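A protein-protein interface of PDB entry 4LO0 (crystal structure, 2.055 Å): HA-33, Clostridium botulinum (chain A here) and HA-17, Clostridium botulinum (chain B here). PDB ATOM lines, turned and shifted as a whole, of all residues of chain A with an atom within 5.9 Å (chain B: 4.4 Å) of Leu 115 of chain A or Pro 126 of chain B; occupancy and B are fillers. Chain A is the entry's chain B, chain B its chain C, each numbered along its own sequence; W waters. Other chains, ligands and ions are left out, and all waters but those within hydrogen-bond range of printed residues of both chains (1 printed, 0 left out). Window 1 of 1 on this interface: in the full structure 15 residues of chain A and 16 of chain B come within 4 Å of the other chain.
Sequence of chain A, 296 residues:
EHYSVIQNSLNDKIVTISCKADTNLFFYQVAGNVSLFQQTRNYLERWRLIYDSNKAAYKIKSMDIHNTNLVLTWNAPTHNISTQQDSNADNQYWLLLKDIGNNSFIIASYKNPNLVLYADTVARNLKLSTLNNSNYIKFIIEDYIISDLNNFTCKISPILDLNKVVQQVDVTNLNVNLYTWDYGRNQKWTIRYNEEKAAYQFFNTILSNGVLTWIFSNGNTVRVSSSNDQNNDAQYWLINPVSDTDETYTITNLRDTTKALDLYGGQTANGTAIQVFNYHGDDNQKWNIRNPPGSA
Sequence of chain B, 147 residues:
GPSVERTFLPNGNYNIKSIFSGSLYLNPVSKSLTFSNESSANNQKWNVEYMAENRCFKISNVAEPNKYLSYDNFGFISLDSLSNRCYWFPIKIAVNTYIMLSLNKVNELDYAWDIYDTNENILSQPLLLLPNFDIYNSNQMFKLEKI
Water W1 bridges O of Pro 126 of chain B (2.8 Å) and ND2 of Asn 112 of chain A (3.1 Å).
Of chain B, only Phe 76 (3.9 Å), Pro 126 (3.8 Å) and Leu 128 (3.7 Å) come within 4 Å of Leu 115 of chain A. Pro 126 of chain B touches three residues of chain A. Of the printed residues of chain A, Leu 128 of chain B touches Asn 112 (3.97 Å) and Leu 115 (3.7 Å). Of the printed residues of chain B, Ala 76 of chain A touches Ser 124 (3.2 Å). Of the printed residues of chain B, Leu 128 of chain A touches Phe 76. Printed residues of chain A within 4 Å of Phe 76 of chain B: Leu 115 (3.9 Å) and Leu 128 (3.9 Å). Thr 78 of chain A touches none of the printed residues of chain B. The nearest printed residue of chain B that does not touch Leu 115 of chain A is Gln 125 of chain B (5.7 Å).
OE1 of Gln 125 of chain B sits at hydrogen-bond distance from ND2 of Asn 112 of chain A (2.9 Å). The backbone nitrogen (N) of Pro 77 of chain A lies close to the backbone carbonyl oxygen (O) of Ser 124 of chain B, 3.3 Å away.
Among the printed residues, pairs that only touch across the chains: Trp 74 of chain A with Gln 125 of chain B (3.99 Å), Trp 74 of chain A with Pro 126 of chain B (3.5 Å), Ala 76 of chain A with Ser 124 of chain B (3.2 Å), Pro 77 of chain A with Gln 125 of chain B (3.9 Å), Pro 77 of chain A with Pro 126 of chain B (3.5 Å), Asn 112 of chain A with Leu 128 of chain B (3.97 Å), Leu 115 of chain A with Phe 76 of chain B (3.9 Å), Leu 115 of chain A with Pro 126 of chain B (3.8 Å), Leu 115 of chain A with Leu 128 of chain B (3.7 Å) and Leu 128 of chain A with Phe 76 of chain B (3.9 Å).
The indole nitrogen (NE1) of Trp 74 of chain A lies within hydrogen-bond range of the backbone carbonyl oxygen (O) of Thr 78 of chain A. The backbone NH (N) of Ser 109 of chain A lies within hydrogen-bond range of the backbone carbonyl oxygen (O) of Leu 115 of chain A, 2.9 Å away. The side-chain amide oxygen of Asn 112 of chain A is in hydrogen-bond range of the side-chain amide nitrogen of Asn 114 of chain A (3.1 Å). O of Leu 128 of chain B sits at hydrogen-bond distance from N of Asp 114 of chain B (2.9 Å).
Of the 18 printed residues of chain A, 6 touch a printed residue of chain B. Hydrophobic or aromatic side chains of chain A that line the printed part of chain B: Trp 74, Ala 76, Pro 77, Leu 115 and Leu 128. Along chain B the printed residues that touch a printed residue of chain A span positions 76 to 128. Among the printed residues, 12 pairs touch across the chains.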
ATOM      1  N   TRP A  74       1.859   9.666 -32.234  1.00  0.00           N
ATOM      2  CA  TRP A  74       0.943   9.548 -31.106  1.00  0.00           C
ATOM      3  C   TRP A  74       0.113   8.293 -31.305  1.00  0.00           C
ATOM      4  O   TRP A  74      -0.607   8.157 -32.302  1.00  0.00           O
ATOM      5  CB  TRP A  74       0.004  10.770 -31.013  1.00  0.00           C
ATOM      6  CG  TRP A  74      -1.151  10.565 -30.051  1.00  0.00           C
ATOM      7  CD1 TRP A  74      -1.153   9.790 -28.921  1.00  0.00           C
ATOM      8  CD2 TRP A  74      -2.473  11.147 -30.138  1.00  0.00           C
ATOM      9  NE1 TRP A  74      -2.383   9.848 -28.306  1.00  0.00           N
ATOM     10  CE2 TRP A  74      -3.210  10.677 -29.024  1.00  0.00           C
ATOM     11  CE3 TRP A  74      -3.095  12.021 -31.044  1.00  0.00           C
ATOM     12  CZ2 TRP A  74      -4.550  11.023 -28.799  1.00  0.00           C
ATOM     13  CZ3 TRP A  74      -4.428  12.383 -30.818  1.00  0.00           C
ATOM     14  CH2 TRP A  74      -5.142  11.880 -29.695  1.00  0.00           C
ATOM     15  N   ALA A  76      -2.743   7.240 -30.575  1.00  0.00           N
ATOM     16  CA  ALA A  76      -4.137   7.536 -30.203  1.00  0.00           C
ATOM     17  C   ALA A  76      -4.956   6.230 -30.148  1.00  0.00           C
ATOM     18  O   ALA A  76      -4.812   5.379 -31.022  1.00  0.00           O
ATOM     19  CB  ALA A  76      -4.757   8.504 -31.208  1.00  0.00           C
ATOM     20  N   PRO A  77      -5.839   6.079 -29.140  1.00  0.00           N
ATOM     21  CA  PRO A  77      -6.242   7.094 -28.159  1.00  0.00           C
ATOM     22  C   PRO A  77      -5.415   7.067 -26.882  1.00  0.00           C
ATOM     23  O   PRO A  77      -5.755   7.785 -25.949  1.00  0.00           O
ATOM     24  CB  PRO A  77      -7.667   6.686 -27.822  1.00  0.00           C
ATOM     25  CG  PRO A  77      -7.594   5.128 -27.881  1.00  0.00           C
ATOM     26  CD  PRO A  77      -6.579   4.807 -28.957  1.00  0.00           C
ATOM     27  N   THR A  78      -4.346   6.273 -26.833  1.00  0.00           N
ATOM     28  CA  THR A  78      -3.604   6.113 -25.579  1.00  0.00           C
ATOM     29  C   THR A  78      -2.763   7.343 -25.234  1.00  0.00           C
ATOM     30  O   THR A  78      -2.653   8.268 -26.026  1.00  0.00           O
ATOM     31  CB  THR A  78      -2.665   4.905 -25.661  1.00  0.00           C
ATOM     32  OG1 THR A  78      -1.523   5.261 -26.444  1.00  0.00           O
ATOM     33  CG2 THR A  78      -3.384   3.719 -26.308  1.00  0.00           C
ATOM     34  N   TRP A  94       2.475  17.225 -36.386  1.00  0.00           N
ATOM     35  CA  TRP A  94       2.594  18.026 -35.179  1.00  0.00           C
ATOM     36  C   TRP A  94       2.592  19.518 -35.556  1.00  0.00           C
ATOM     37  O   TRP A  94       3.201  19.907 -36.551  1.00  0.00           O
ATOM     38  CB  TRP A  94       3.895  17.653 -34.467  1.00  0.00           C
ATOM     39  CG  TRP A  94       3.920  16.176 -34.104  1.00  0.00           C
ATOM     40  CD1 TRP A  94       4.488  15.143 -34.826  1.00  0.00           C
ATOM     41  CD2 TRP A  94       3.308  15.582 -32.960  1.00  0.00           C
ATOM     42  NE1 TRP A  94       4.272  13.941 -34.171  1.00  0.00           N
ATOM     43  CE2 TRP A  94       3.545  14.186 -33.028  1.00  0.00           C
ATOM     44  CE3 TRP A  94       2.569  16.093 -31.879  1.00  0.00           C
ATOM     45  CZ2 TRP A  94       3.078  13.299 -32.050  1.00  0.00           C
ATOM     46  CZ3 TRP A  94       2.104  15.202 -30.902  1.00  0.00           C
ATOM     47  CH2 TRP A  94       2.358  13.826 -31.002  1.00  0.00           C
ATOM     48  N   ILE A 107       4.325  21.579 -28.793  1.00  0.00           N
ATOM     49  CA  ILE A 107       4.228  20.640 -29.897  1.00  0.00           C
ATOM     50  C   ILE A 107       2.900  19.908 -29.817  1.00  0.00           C
ATOM     51  O   ILE A 107       2.732  18.987 -29.020  1.00  0.00           O
ATOM     52  CB  ILE A 107       5.403  19.638 -29.830  1.00  0.00           C
ATOM     53  CG1 ILE A 107       6.728  20.413 -29.794  1.00  0.00           C
ATOM     54  CG2 ILE A 107       5.349  18.702 -31.018  1.00  0.00           C
ATOM     55  CD1 ILE A 107       8.005  19.483 -29.816  1.00  0.00           C
ATOM     56  N   ALA A 108       1.947  20.354 -30.628  1.00  0.00           N
ATOM     57  CA  ALA A 108       0.559  19.926 -30.531  1.00  0.00           C
ATOM     58  C   ALA A 108       0.249  18.878 -31.587  1.00  0.00           C
ATOM     59  O   ALA A 108       0.699  18.984 -32.735  1.00  0.00           O
ATOM     60  CB  ALA A 108      -0.384  21.153 -30.694  1.00  0.00           C
ATOM     61  N   SER A 109      -0.540  17.867 -31.223  1.00  0.00           N
ATOM     62  CA  SER A 109      -0.912  16.858 -32.204  1.00  0.00           C
ATOM     63  C   SER A 109      -1.799  17.420 -33.278  1.00  0.00           C
ATOM     64  O   SER A 109      -2.815  18.054 -32.979  1.00  0.00           O
ATOM     65  CB  SER A 109      -1.673  15.698 -31.558  1.00  0.00           C
ATOM     66  OG  SER A 109      -1.985  14.760 -32.584  1.00  0.00           O
ATOM     67  N   ASN A 112      -5.296  15.854 -32.937  1.00  0.00           N
ATOM     68  CA  ASN A 112      -6.116  16.466 -31.876  1.00  0.00           C
ATOM     69  C   ASN A 112      -5.304  17.568 -31.242  1.00  0.00           C
ATOM     70  O   ASN A 112      -4.572  17.328 -30.290  1.00  0.00           O
ATOM     71  CB  ASN A 112      -6.520  15.453 -30.792  1.00  0.00           C
ATOM     72  CG  ASN A 112      -7.582  16.009 -29.839  1.00  0.00           C
ATOM     73  OD1 ASN A 112      -7.698  17.230 -29.643  1.00  0.00           O
ATOM     74  ND2 ASN A 112      -8.370  15.116 -29.252  1.00  0.00           N
ATOM     75  N   PRO A 113      -5.441  18.796 -31.771  1.00  0.00           N
ATOM     76  CA  PRO A 113      -4.653  19.971 -31.362  1.00  0.00           C
ATOM     77  C   PRO A 113      -4.917  20.435 -29.925  1.00  0.00           C
ATOM     78  O   PRO A 113      -4.156  21.260 -29.415  1.00  0.00           O
ATOM     79  CB  PRO A 113      -5.058  21.059 -32.372  1.00  0.00           C
ATOM     80  CG  PRO A 113      -5.885  20.406 -33.390  1.00  0.00           C
ATOM     81  CD  PRO A 113      -6.378  19.090 -32.862  1.00  0.00           C
ATOM     82  N   ASN A 114      -5.958  19.926 -29.271  1.00  0.00           N
ATOM     83  CA  ASN A 114      -6.075  20.113 -27.815  1.00  0.00           C
ATOM     84  C   ASN A 114      -4.988  19.413 -27.004  1.00  0.00           C
ATOM     85  O   ASN A 114      -4.786  19.722 -25.824  1.00  0.00           O
ATOM     86  CB  ASN A 114      -7.442  19.641 -27.309  1.00  0.00           C
ATOM     87  CG  ASN A 114      -8.573  20.427 -27.932  1.00  0.00           C
ATOM     88  OD1 ASN A 114      -8.764  21.609 -27.622  1.00  0.00           O
ATOM     89  ND2 ASN A 114      -9.324  19.788 -28.822  1.00  0.00           N
ATOM     90  N   LEU A 115      -4.302  18.460 -27.623  1.00  0.00           N
ATOM     91  CA  LEU A 115      -3.299  17.679 -26.895  1.00  0.00           C
ATOM     92  C   LEU A 115      -1.894  17.999 -27.382  1.00  0.00           C
ATOM     93  O   LEU A 115      -1.640  18.054 -28.590  1.00  0.00           O
ATOM     94  CB  LEU A 115      -3.559  16.173 -27.073  1.00  0.00           C
ATOM     95  CG  LEU A 115      -4.908  15.719 -26.502  1.00  0.00           C
ATOM     96  CD1 LEU A 115      -5.138  14.203 -26.814  1.00  0.00           C
ATOM     97  CD2 LEU A 115      -4.943  15.973 -24.971  1.00  0.00           C
ATOM     98  N   VAL A 116      -0.982  18.197 -26.438  1.00  0.00           N
ATOM     99  CA  VAL A 116       0.396  18.544 -26.775  1.00  0.00           C
ATOM    100  C   VAL A 116       1.359  17.618 -26.029  1.00  0.00           C
ATOM    101  O   VAL A 116       0.988  17.007 -25.017  1.00  0.00           O
ATOM    102  CB  VAL A 116       0.698  20.016 -26.420  1.00  0.00           C
ATOM    103  CG1 VAL A 116      -0.398  20.941 -26.995  1.00  0.00           C
ATOM    104  CG2 VAL A 116       0.778  20.173 -24.886  1.00  0.00           C
ATOM    105  N   LEU A 117       2.588  17.514 -26.536  1.00  0.00           N
ATOM    106  CA  LEU A 117       3.602  16.699 -25.899  1.00  0.00           C
ATOM    107  C   LEU A 117       3.865  17.222 -24.488  1.00  0.00           C
ATOM    108  O   LEU A 117       3.913  18.439 -24.234  1.00  0.00           O
ATOM    109  CB  LEU A 117       4.890  16.711 -26.718  1.00  0.00           C
ATOM    110  CG  LEU A 117       4.821  15.960 -28.051  1.00  0.00           C
ATOM    111  CD1 LEU A 117       6.184  15.993 -28.791  1.00  0.00           C
ATOM    112  CD2 LEU A 117       4.359  14.511 -27.831  1.00  0.00           C
ATOM    113  N   LEU A 128       0.967  13.037 -23.070  1.00  0.00           N
ATOM    114  CA  LEU A 128       0.206  14.137 -23.663  1.00  0.00           C
ATOM    115  C   LEU A 128      -0.509  14.898 -22.581  1.00  0.00           C
ATOM    116  O   LEU A 128      -0.715  14.393 -21.484  1.00  0.00           O
ATOM    117  CB  LEU A 128      -0.816  13.637 -24.687  1.00  0.00           C
ATOM    118  CG  LEU A 128      -0.230  13.114 -25.998  1.00  0.00           C
ATOM    119  CD1 LEU A 128      -1.330  12.517 -26.813  1.00  0.00           C
ATOM    120  CD2 LEU A 128       0.435  14.258 -26.794  1.00  0.00           C
ATOM    121  N   SER A 129      -0.883  16.135 -22.893  1.00  0.00           N
ATOM    122  CA  SER A 129      -1.606  16.957 -21.937  1.00  0.00           C
ATOM    123  C   SER A 129      -2.392  17.958 -22.728  1.00  0.00           C
ATOM    124  O   SER A 129      -2.029  18.300 -23.859  1.00  0.00           O
ATOM    125  CB  SER A 129      -0.616  17.672 -21.025  1.00  0.00           C
ATOM    126  OG  SER A 129      -1.255  18.558 -20.129  1.00  0.00           O
ATOM    127  N   THR A 130      -3.480  18.430 -22.144  1.00  0.00           N
ATOM    128  CA  THR A 130      -4.084  19.630 -22.671  1.00  0.00           C
ATOM    129  C   THR A 130      -3.144  20.786 -22.324  1.00  0.00           C
ATOM    130  O   THR A 130      -2.205  20.623 -21.526  1.00  0.00           O
ATOM    131  CB  THR A 130      -5.516  19.853 -22.133  1.00  0.00           C
ATOM    132  OG1 THR A 130      -5.513  19.731 -20.709  1.00  0.00           O
ATOM    133  CG2 THR A 130      -6.455  18.827 -22.725  1.00  0.00           C
ATOM    134  N   LEU A 131      -3.375  21.938 -22.948  1.00  0.00           N
ATOM    135  CA  LEU A 131      -2.485  23.093 -22.788  1.00  0.00           C
ATOM    136  C   LEU A 131      -2.575  23.673 -21.395  1.00  0.00           C
ATOM    137  O   LEU A 131      -3.656  23.812 -20.839  1.00  0.00           O
ATOM    138  CB  LEU A 131      -2.909  24.219 -23.719  1.00  0.00           C
ATOM    139  CG  LEU A 131      -2.276  24.449 -25.069  1.00  0.00           C
ATOM    140  CD1 LEU A 131      -0.759  24.529 -24.919  1.00  0.00           C
ATOM    141  CD2 LEU A 131      -2.706  23.327 -25.968  1.00  0.00           C
ATOM    142  N   LEU B  33     -10.125   6.523 -22.658  1.00  0.00           N
ATOM    143  CA  LEU B  33     -11.492   6.170 -23.031  1.00  0.00           C
ATOM    144  C   LEU B  33     -11.678   6.560 -24.493  1.00  0.00           C
ATOM    145  O   LEU B  33     -11.288   7.664 -24.925  1.00  0.00           O
ATOM    146  CB  LEU B  33     -12.537   6.905 -22.158  1.00  0.00           C
ATOM    147  CG  LEU B  33     -12.826   6.398 -20.735  1.00  0.00           C
ATOM    148  CD1 LEU B  33     -13.371   4.953 -20.725  1.00  0.00           C
ATOM    149  CD2 LEU B  33     -11.590   6.484 -19.840  1.00  0.00           C
ATOM    150  N   PHE B  76      -7.473  14.218 -19.661  1.00  0.00           N
ATOM    151  CA  PHE B  76      -8.155  13.029 -20.162  1.00  0.00           C
ATOM    152  C   PHE B  76      -9.217  12.520 -19.178  1.00  0.00           C
ATOM    153  O   PHE B  76      -9.007  12.556 -17.965  1.00  0.00           O
ATOM    154  CB  PHE B  76      -7.173  11.857 -20.334  1.00  0.00           C
ATOM    155  CG  PHE B  76      -6.206  12.001 -21.472  1.00  0.00           C
ATOM    156  CD1 PHE B  76      -5.164  12.911 -21.410  1.00  0.00           C
ATOM    157  CD2 PHE B  76      -6.311  11.178 -22.583  1.00  0.00           C
ATOM    158  CE1 PHE B  76      -4.256  13.025 -22.461  1.00  0.00           C
ATOM    159  CE2 PHE B  76      -5.397  11.264 -23.628  1.00  0.00           C
ATOM    160  CZ  PHE B  76      -4.369  12.191 -23.572  1.00  0.00           C
ATOM    161  N   ASP B 114     -15.611  15.757 -23.676  1.00  0.00           N
ATOM    162  CA  ASP B 114     -15.467  16.376 -24.984  1.00  0.00           C
ATOM    163  C   ASP B 114     -14.719  15.411 -25.885  1.00  0.00           C
ATOM    164  O   ASP B 114     -13.666  14.915 -25.520  1.00  0.00           O
ATOM    165  CB  ASP B 114     -14.679  17.671 -24.818  1.00  0.00           C
ATOM    166  CG  ASP B 114     -14.688  18.550 -26.077  1.00  0.00           C
ATOM    167  OD1 ASP B 114     -14.289  18.068 -27.169  1.00  0.00           O
ATOM    168  OD2 ASP B 114     -15.101  19.735 -25.965  1.00  0.00           O
ATOM    169  N   ILE B 115     -15.270  15.132 -27.055  1.00  0.00           N
ATOM    170  CA  ILE B 115     -14.616  14.234 -27.994  1.00  0.00           C
ATOM    171  C   ILE B 115     -14.361  15.014 -29.277  1.00  0.00           C
ATOM    172  O   ILE B 115     -15.291  15.603 -29.851  1.00  0.00           O
ATOM    173  CB  ILE B 115     -15.472  12.964 -28.275  1.00  0.00           C
ATOM    174  CG1 ILE B 115     -14.688  11.942 -29.125  1.00  0.00           C
ATOM    175  CG2 ILE B 115     -16.846  13.312 -28.859  1.00  0.00           C
ATOM    176  CD1 ILE B 115     -13.719  11.112 -28.285  1.00  0.00           C
ATOM    177  N   SER B 124     -10.452   6.593 -32.797  1.00  0.00           N
ATOM    178  CA  SER B 124      -9.169   6.663 -32.091  1.00  0.00           C
ATOM    179  C   SER B 124      -8.947   7.931 -31.270  1.00  0.00           C
ATOM    180  O   SER B 124      -7.854   8.113 -30.723  1.00  0.00           O
ATOM    181  CB  SER B 124      -7.978   6.488 -33.052  1.00  0.00           C
ATOM    182  OG  SER B 124      -8.242   5.503 -34.023  1.00  0.00           O
ATOM    183  N   GLN B 125      -9.957   8.797 -31.172  1.00  0.00           N
ATOM    184  CA  GLN B 125      -9.833   9.968 -30.309  1.00  0.00           C
ATOM    185  C   GLN B 125     -10.059   9.575 -28.851  1.00  0.00           C
ATOM    186  O   GLN B 125     -10.957   8.795 -28.557  1.00  0.00           O
ATOM    187  CB  GLN B 125     -10.855  11.055 -30.685  1.00  0.00           C
ATOM    188  CG  GLN B 125     -10.595  11.730 -32.022  1.00  0.00           C
ATOM    189  CD  GLN B 125      -9.372  12.613 -32.007  1.00  0.00           C
ATOM    190  OE1 GLN B 125      -8.799  12.870 -30.955  1.00  0.00           O
ATOM    191  NE2 GLN B 125      -8.951  13.073 -33.189  1.00  0.00           N
ATOM    192  N   PRO B 126      -9.272  10.148 -27.933  1.00  0.00           N
ATOM    193  CA  PRO B 126      -9.559   9.899 -26.519  1.00  0.00           C
ATOM    194  C   PRO B 126     -10.614  10.887 -26.033  1.00  0.00           C
ATOM    195  O   PRO B 126     -10.665  12.034 -26.512  1.00  0.00           O
ATOM    196  CB  PRO B 126      -8.230  10.203 -25.838  1.00  0.00           C
ATOM    197  CG  PRO B 126      -7.596  11.320 -26.736  1.00  0.00           C
ATOM    198  CD  PRO B 126      -8.117  11.054 -28.134  1.00  0.00           C
ATOM    199  N   LEU B 127     -11.435  10.463 -25.084  1.00  0.00           N
ATOM    200  CA  LEU B 127     -12.408  11.361 -24.493  1.00  0.00           C
ATOM    201  C   LEU B 127     -11.676  12.275 -23.511  1.00  0.00           C
ATOM    202  O   LEU B 127     -10.931  11.798 -22.649  1.00  0.00           O
ATOM    203  CB  LEU B 127     -13.524  10.561 -23.819  1.00  0.00           C
ATOM    204  CG  LEU B 127     -14.719  11.354 -23.269  1.00  0.00           C
ATOM    205  CD1 LEU B 127     -15.471  12.014 -24.409  1.00  0.00           C
ATOM    206  CD2 LEU B 127     -15.654  10.419 -22.457  1.00  0.00           C
ATOM    207  N   LEU B 128     -11.865  13.593 -23.664  1.00  0.00           N
ATOM    208  CA  LEU B 128     -11.175  14.566 -22.825  1.00  0.00           C
ATOM    209  C   LEU B 128     -12.160  15.293 -21.891  1.00  0.00           C
ATOM    210  O   LEU B 128     -13.373  15.078 -21.956  1.00  0.00           O
ATOM    211  CB  LEU B 128     -10.375  15.570 -23.690  1.00  0.00           C
ATOM    212  CG  LEU B 128      -9.382  15.012 -24.719  1.00  0.00           C
ATOM    213  CD1 LEU B 128      -8.603  16.144 -25.428  1.00  0.00           C
ATOM    214  CD2 LEU B 128      -8.414  14.000 -24.056  1.00  0.00           C
HETATM  215  O   HOH W   1     -11.113  14.303 -28.037  1.00  0.00           O
